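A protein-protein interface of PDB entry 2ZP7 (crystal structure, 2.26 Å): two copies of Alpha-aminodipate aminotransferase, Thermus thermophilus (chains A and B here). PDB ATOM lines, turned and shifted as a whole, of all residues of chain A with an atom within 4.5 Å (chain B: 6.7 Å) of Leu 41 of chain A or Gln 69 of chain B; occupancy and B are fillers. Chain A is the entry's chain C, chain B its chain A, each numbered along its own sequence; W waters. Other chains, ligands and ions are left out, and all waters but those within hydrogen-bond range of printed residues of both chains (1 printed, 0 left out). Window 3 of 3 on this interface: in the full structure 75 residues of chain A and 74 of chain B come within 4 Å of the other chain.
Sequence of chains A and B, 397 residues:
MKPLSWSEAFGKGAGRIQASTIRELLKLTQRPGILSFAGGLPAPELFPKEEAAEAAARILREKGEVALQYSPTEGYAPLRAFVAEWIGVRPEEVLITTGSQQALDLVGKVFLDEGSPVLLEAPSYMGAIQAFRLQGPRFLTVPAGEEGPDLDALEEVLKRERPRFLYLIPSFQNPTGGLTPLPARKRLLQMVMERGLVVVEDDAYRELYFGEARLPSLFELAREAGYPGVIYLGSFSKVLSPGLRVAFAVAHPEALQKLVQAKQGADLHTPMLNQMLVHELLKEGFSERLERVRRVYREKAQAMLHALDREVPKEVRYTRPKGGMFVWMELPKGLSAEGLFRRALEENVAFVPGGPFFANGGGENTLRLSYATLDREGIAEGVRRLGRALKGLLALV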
ATOM      1  N   LEU A  25     -11.811  18.691 -18.694  1.00  0.00           N
ATOM      2  CA  LEU A  25     -10.705  18.130 -19.477  1.00  0.00           C
ATOM      3  C   LEU A  25     -10.359  16.750 -18.921  1.00  0.00           C
ATOM      4  O   LEU A  25     -10.646  15.742 -19.558  1.00  0.00           O
ATOM      5  CB  LEU A  25      -9.472  19.057 -19.414  1.00  0.00           C
ATOM      6  CG  LEU A  25      -8.202  18.882 -20.267  1.00  0.00           C
ATOM      7  CD1 LEU A  25      -7.251  20.053 -20.017  1.00  0.00           C
ATOM      8  CD2 LEU A  25      -7.474  17.553 -20.029  1.00  0.00           C
ATOM      9  N   LEU A  28     -12.095  13.408 -19.450  1.00  0.00           N
ATOM     10  CA  LEU A  28     -12.253  12.984 -20.853  1.00  0.00           C
ATOM     11  C   LEU A  28     -12.223  11.473 -21.099  1.00  0.00           C
ATOM     12  O   LEU A  28     -12.060  11.022 -22.242  1.00  0.00           O
ATOM     13  CB  LEU A  28     -11.262  13.719 -21.774  1.00  0.00           C
ATOM     14  CG  LEU A  28      -9.762  13.407 -21.848  1.00  0.00           C
ATOM     15  CD1 LEU A  28      -9.076  14.579 -22.520  1.00  0.00           C
ATOM     16  CD2 LEU A  28      -9.130  13.134 -20.481  1.00  0.00           C
ATOM     17  N   GLY A  39      -6.863  18.346 -24.529  1.00  0.00           N
ATOM     18  CA  GLY A  39      -6.073  17.818 -23.413  1.00  0.00           C
ATOM     19  C   GLY A  39      -4.813  17.157 -23.909  1.00  0.00           C
ATOM     20  O   GLY A  39      -4.854  16.267 -24.767  1.00  0.00           O
ATOM     21  N   GLY A  40      -3.689  17.612 -23.367  1.00  0.00           N
ATOM     22  CA  GLY A  40      -2.382  17.100 -23.729  1.00  0.00           C
ATOM     23  C   GLY A  40      -2.065  15.875 -22.909  1.00  0.00           C
ATOM     24  O   GLY A  40      -1.171  15.906 -22.067  1.00  0.00           O
ATOM     25  N   LEU A  41      -2.813  14.802 -23.157  1.00  0.00           N
ATOM     26  CA  LEU A  41      -2.590  13.533 -22.494  1.00  0.00           C
ATOM     27  C   LEU A  41      -1.539  12.727 -23.254  1.00  0.00           C
ATOM     28  O   LEU A  41      -1.777  12.326 -24.404  1.00  0.00           O
ATOM     29  CB  LEU A  41      -3.902  12.758 -22.372  1.00  0.00           C
ATOM     30  CG  LEU A  41      -4.775  13.023 -21.134  1.00  0.00           C
ATOM     31  CD1 LEU A  41      -5.439  14.396 -21.199  1.00  0.00           C
ATOM     32  CD2 LEU A  41      -5.805  11.947 -20.996  1.00  0.00           C
ATOM     33  N   PRO A  42      -0.359  12.503 -22.624  1.00  0.00           N
ATOM     34  CA  PRO A  42       0.722  11.734 -23.241  1.00  0.00           C
ATOM     35  C   PRO A  42       0.242  10.407 -23.814  1.00  0.00           C
ATOM     36  O   PRO A  42      -0.670   9.779 -23.270  1.00  0.00           O
ATOM     37  CB  PRO A  42       1.687  11.475 -22.076  1.00  0.00           C
ATOM     38  CG  PRO A  42       1.464  12.557 -21.159  1.00  0.00           C
ATOM     39  CD  PRO A  42       0.020  12.975 -21.282  1.00  0.00           C
ATOM     40  N   ALA A  43       0.875   9.998 -24.906  1.00  0.00           N
ATOM     41  CA  ALA A  43       0.501   8.806 -25.632  1.00  0.00           C
ATOM     42  C   ALA A  43       0.690   7.598 -24.719  1.00  0.00           C
ATOM     43  O   ALA A  43       1.807   7.354 -24.246  1.00  0.00           O
ATOM     44  CB  ALA A  43       1.358   8.681 -26.906  1.00  0.00           C
ATOM     45  N   PHE A  47       3.841   4.471 -22.279  1.00  0.00           N
ATOM     46  CA  PHE A  47       3.886   4.041 -20.872  1.00  0.00           C
ATOM     47  C   PHE A  47       4.678   2.736 -20.666  1.00  0.00           C
ATOM     48  O   PHE A  47       4.356   1.706 -21.251  1.00  0.00           O
ATOM     49  CB  PHE A  47       2.469   3.870 -20.308  1.00  0.00           C
ATOM     50  CG  PHE A  47       1.671   5.168 -20.185  1.00  0.00           C
ATOM     51  CD1 PHE A  47       2.293   6.416 -20.209  1.00  0.00           C
ATOM     52  CD2 PHE A  47       0.291   5.120 -19.995  1.00  0.00           C
ATOM     53  CE1 PHE A  47       1.550   7.579 -20.104  1.00  0.00           C
ATOM     54  CE2 PHE A  47      -0.451   6.284 -19.854  1.00  0.00           C
ATOM     55  CZ  PHE A  47       0.166   7.510 -19.919  1.00  0.00           C
ATOM     56  N   PRO A 242       2.342  11.319 -16.690  1.00  0.00           N
ATOM     57  CA  PRO A 242       1.706  12.446 -16.000  1.00  0.00           C
ATOM     58  C   PRO A 242       1.008  12.033 -14.692  1.00  0.00           C
ATOM     59  O   PRO A 242       0.961  12.813 -13.748  1.00  0.00           O
ATOM     60  CB  PRO A 242       0.680  12.928 -17.026  1.00  0.00           C
ATOM     61  CG  PRO A 242       0.355  11.726 -17.833  1.00  0.00           C
ATOM     62  CD  PRO A 242       1.617  10.940 -17.919  1.00  0.00           C
ATOM     63  N   GLY A 243       0.469  10.817 -14.646  1.00  0.00           N
ATOM     64  CA  GLY A 243      -0.262  10.323 -13.481  1.00  0.00           C
ATOM     65  C   GLY A 243       0.512  10.207 -12.178  1.00  0.00           C
ATOM     66  O   GLY A 243      -0.079  10.308 -11.101  1.00  0.00           O
ATOM     67  N   ALA A 372      -1.653  14.216 -29.188  1.00  0.00           N
ATOM     68  CA  ALA A 372      -0.830  13.434 -28.254  1.00  0.00           C
ATOM     69  C   ALA A 372      -1.335  12.025 -27.912  1.00  0.00           C
ATOM     70  O   ALA A 372      -0.534  11.096 -27.740  1.00  0.00           O
ATOM     71  CB  ALA A 372      -0.597  14.240 -26.966  1.00  0.00           C
ATOM     72  N   THR A 373      -2.650  11.877 -27.790  1.00  0.00           N
ATOM     73  CA  THR A 373      -3.244  10.710 -27.137  1.00  0.00           C
ATOM     74  C   THR A 373      -3.726   9.636 -28.110  1.00  0.00           C
ATOM     75  O   THR A 373      -3.534   8.444 -27.863  1.00  0.00           O
ATOM     76  CB  THR A 373      -4.435  11.136 -26.278  1.00  0.00           C
ATOM     77  OG1 THR A 373      -4.142  12.394 -25.660  1.00  0.00           O
ATOM     78  CG2 THR A 373      -4.727  10.079 -25.213  1.00  0.00           C
ATOM     79  N   GLY B  64      -2.205  -0.103 -15.849  1.00  0.00           N
ATOM     80  CA  GLY B  64      -1.143   0.875 -15.996  1.00  0.00           C
ATOM     81  C   GLY B  64      -1.534   2.096 -16.805  1.00  0.00           C
ATOM     82  O   GLY B  64      -0.989   3.176 -16.581  1.00  0.00           O
ATOM     83  N   GLU B  65      -2.472   1.937 -17.741  1.00  0.00           N
ATOM     84  CA  GLU B  65      -2.924   3.058 -18.546  1.00  0.00           C
ATOM     85  C   GLU B  65      -3.765   4.082 -17.758  1.00  0.00           C
ATOM     86  O   GLU B  65      -3.649   5.274 -17.995  1.00  0.00           O
ATOM     87  CB  GLU B  65      -3.584   2.593 -19.860  1.00  0.00           C
ATOM     88  CG  GLU B  65      -4.935   1.839 -19.724  1.00  0.00           C
ATOM     89  CD  GLU B  65      -4.886   0.626 -18.791  1.00  0.00           C
ATOM     90  OE1 GLU B  65      -5.675   0.640 -17.814  1.00  0.00           O
ATOM     91  OE2 GLU B  65      -4.069  -0.311 -19.027  1.00  0.00           O
ATOM     92  N   VAL B  66      -4.552   3.625 -16.790  1.00  0.00           N
ATOM     93  CA  VAL B  66      -5.208   4.518 -15.820  1.00  0.00           C
ATOM     94  C   VAL B  66      -4.266   5.029 -14.710  1.00  0.00           C
ATOM     95  O   VAL B  66      -4.282   6.235 -14.362  1.00  0.00           O
ATOM     96  CB  VAL B  66      -6.486   3.864 -15.230  1.00  0.00           C
ATOM     97  CG1 VAL B  66      -6.234   2.391 -14.922  1.00  0.00           C
ATOM     98  CG2 VAL B  66      -7.003   4.602 -13.985  1.00  0.00           C
ATOM     99  N   ALA B  67      -3.439   4.132 -14.172  1.00  0.00           N
ATOM    100  CA  ALA B  67      -2.523   4.483 -13.100  1.00  0.00           C
ATOM    101  C   ALA B  67      -1.509   5.545 -13.508  1.00  0.00           C
ATOM    102  O   ALA B  67      -1.103   6.358 -12.680  1.00  0.00           O
ATOM    103  CB  ALA B  67      -1.808   3.241 -12.572  1.00  0.00           C
ATOM    104  N   LEU B  68      -1.127   5.550 -14.783  1.00  0.00           N
ATOM    105  CA  LEU B  68      -0.001   6.355 -15.271  1.00  0.00           C
ATOM    106  C   LEU B  68      -0.438   7.634 -16.006  1.00  0.00           C
ATOM    107  O   LEU B  68       0.387   8.511 -16.281  1.00  0.00           O
ATOM    108  CB  LEU B  68       0.896   5.500 -16.192  1.00  0.00           C
ATOM    109  CG  LEU B  68       2.203   4.856 -15.681  1.00  0.00           C
ATOM    110  CD1 LEU B  68       2.353   4.820 -14.155  1.00  0.00           C
ATOM    111  CD2 LEU B  68       2.520   3.477 -16.318  1.00  0.00           C
ATOM    112  N   GLN B  69      -1.727   7.721 -16.317  1.00  0.00           N
ATOM    113  CA  GLN B  69      -2.293   8.806 -17.114  1.00  0.00           C
ATOM    114  C   GLN B  69      -2.871   9.897 -16.194  1.00  0.00           C
ATOM    115  O   GLN B  69      -3.222   9.611 -15.031  1.00  0.00           O
ATOM    116  CB  GLN B  69      -3.403   8.227 -18.013  1.00  0.00           C
ATOM    117  CG  GLN B  69      -4.011   9.164 -19.079  1.00  0.00           C
ATOM    118  CD  GLN B  69      -2.940   9.821 -19.871  1.00  0.00           C
ATOM    119  OE1 GLN B  69      -2.242  10.688 -19.351  1.00  0.00           O
ATOM    120  NE2 GLN B  69      -2.739   9.375 -21.110  1.00  0.00           N
ATOM    121  N   TYR B  70      -2.966  11.138 -16.703  1.00  0.00           N
ATOM    122  CA  TYR B  70      -3.779  12.172 -16.037  1.00  0.00           C
ATOM    123  C   TYR B  70      -5.164  11.600 -15.751  1.00  0.00           C
ATOM    124  O   TYR B  70      -5.672  10.772 -16.490  1.00  0.00           O
ATOM    125  CB  TYR B  70      -3.954  13.426 -16.872  1.00  0.00           C
ATOM    126  CG  TYR B  70      -2.760  14.362 -16.936  1.00  0.00           C
ATOM    127  CD1 TYR B  70      -2.208  14.927 -15.781  1.00  0.00           C
ATOM    128  CD2 TYR B  70      -2.219  14.729 -18.169  1.00  0.00           C
ATOM    129  CE1 TYR B  70      -1.121  15.800 -15.856  1.00  0.00           C
ATOM    130  CE2 TYR B  70      -1.144  15.597 -18.254  1.00  0.00           C
ATOM    131  CZ  TYR B  70      -0.594  16.128 -17.098  1.00  0.00           C
ATOM    132  OH  TYR B  70       0.463  17.000 -17.215  1.00  0.00           O
ATOM    133  N   SER B  71      -5.766  12.087 -14.677  1.00  0.00           N
ATOM    134  CA  SER B  71      -6.935  11.492 -14.084  1.00  0.00           C
ATOM    135  C   SER B  71      -7.806  12.611 -13.456  1.00  0.00           C
ATOM    136  O   SER B  71      -7.340  13.745 -13.317  1.00  0.00           O
ATOM    137  CB  SER B  71      -6.458  10.478 -13.046  1.00  0.00           C
ATOM    138  OG  SER B  71      -7.349  10.470 -11.958  1.00  0.00           O
ATOM    139  N   HIS B 269      -4.252  16.711  -9.819  1.00  0.00           N
ATOM    140  CA  HIS B 269      -4.921  15.622  -9.141  1.00  0.00           C
ATOM    141  C   HIS B 269      -3.921  14.869  -8.270  1.00  0.00           C
ATOM    142  O   HIS B 269      -2.688  14.958  -8.470  1.00  0.00           O
ATOM    143  CB  HIS B 269      -5.594  14.649 -10.161  1.00  0.00           C
ATOM    144  CG  HIS B 269      -4.616  13.843 -10.959  1.00  0.00           C
ATOM    145  ND1 HIS B 269      -4.232  14.187 -12.238  1.00  0.00           N
ATOM    146  CD2 HIS B 269      -3.951  12.702 -10.664  1.00  0.00           C
ATOM    147  CE1 HIS B 269      -3.348  13.307 -12.688  1.00  0.00           C
ATOM    148  NE2 HIS B 269      -3.168  12.390 -11.756  1.00  0.00           N
ATOM    149  N   MET B 272      -2.496   8.977  -9.211  1.00  0.00           N
ATOM    150  CA  MET B 272      -3.478   7.904  -9.367  1.00  0.00           C
ATOM    151  C   MET B 272      -3.046   6.512  -8.828  1.00  0.00           C
ATOM    152  O   MET B 272      -3.841   5.831  -8.186  1.00  0.00           O
ATOM    153  CB  MET B 272      -3.892   7.814 -10.836  1.00  0.00           C
ATOM    154  CG  MET B 272      -5.149   7.019 -11.052  1.00  0.00           C
ATOM    155  SD  MET B 272      -6.548   7.961 -10.431  1.00  0.00           S
ATOM    156  CE  MET B 272      -7.816   7.249 -11.465  1.00  0.00           C
HETATM  157  O   HOH W   1       0.065   7.617 -10.584  1.00  0.00           O
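Water W1 lies within hydrogen-bond range of O of Ala 67 of chain B (2.7 Å), O of Gly 243 of chain A (2.7 Å) and N of Met 272 of chain B (3.2 Å).
No position is printed for both chains.
Of the 13 pairs that touch across the chains among the printed residues, none has its exchanged pair printed and touching as well.
Gly 40 of chain A touches Tyr 70 of chain B.
Leu 41 of chain A touches Gln 69 of chain B.
Phe 47 of chain A touches Glu 65 of chain B (CE2 to O, 3.8 Å).
Phe 47 of chain A touches Leu 68 of chain B.
Phe 47 of chain A touches Gln 69 of chain B.
Gln 69 of chain B touches Pro 242 of chain A (OE1 to CG, 3.2 Å).
Pro 242 of chain A touches Tyr 70 of chain B (CB to CZ, 3.4 Å).
Gly 243 of chain A touches Gln 69 of chain B (CA to O, 3.4 Å).
His 269 of chain B touches Gly 243 of chain A (NE2 to O, 3.8 Å).
Of chain B, only Gln 69 (3.7 Å) comes within 4 Å of Leu 41 of chain A.
Printed residues of chain B within 4 Å of Phe 47 of chain A: Glu 65, Leu 68 and Gln 69.
Printed residues of chain B within 4 Å of Gly 243 of chain A: Leu 68 (2.8 Å), Gln 69 (3.4 Å), His 269 (3.8 Å) and Met 272 (3.3 Å).
Of the printed residues of chain A, Gln 69 of chain B touches Leu 41, Pro 42, Phe 47, Pro 242 and Gly 243.
Of the printed residues of chain A, Tyr 70 of chain B touches Gly 40 and Pro 242.
Printed residues of chain A within 4 Å of His 269 of chain B: Gly 243.
The nearest printed residue of chain A that does not touch Gln 69 of chain B is Thr 373 of chain A (4.6 Å).
The nearest printed residue of chain A that does not touch Leu 68 of chain B is Pro 42 of chain A (6.4 Å).
N of Met 272 of chain B sits at hydrogen-bond distance from O of Gly 243 of chain A, at 3.3 Å.
The backbone NH (N) of Gly 243 of chain A is in hydrogen-bond range of the backbone carbonyl oxygen (O) of Leu 68 of chain B (2.8 Å).
The side-chain amide nitrogen of Gln 69 of chain B lies within hydrogen-bond range of the backbone carbonyl oxygen of Pro 42 of chain A, 3.0 Å away.
The backbone nitrogen of Pro 242 of chain A sits close to the backbone carbonyl oxygen of Leu 68 of chain B (3.4 Å).
Among the printed residues, no Asp or Glu carboxylate lies within 4 Å of a Lys or Arg side-chain nitrogen of the other chain.
A ring nitrogen (ND1) of His 269 of chain B sits at hydrogen-bond distance from the backbone carbonyl oxygen (O) of Ser 71 of chain B, 3.3 Å away.
The side-chain hydroxyl (OG1) of Thr 373 of chain A is in hydrogen-bond range of the backbone carbonyl oxygen (O) of Leu 41 of chain A (2.7 Å).
The side-chain hydroxyl (OG) of Ser 71 of chain B sits at hydrogen-bond distance from the side-chain sulfur (SD) of Met 272 of chain B (3.0 Å).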
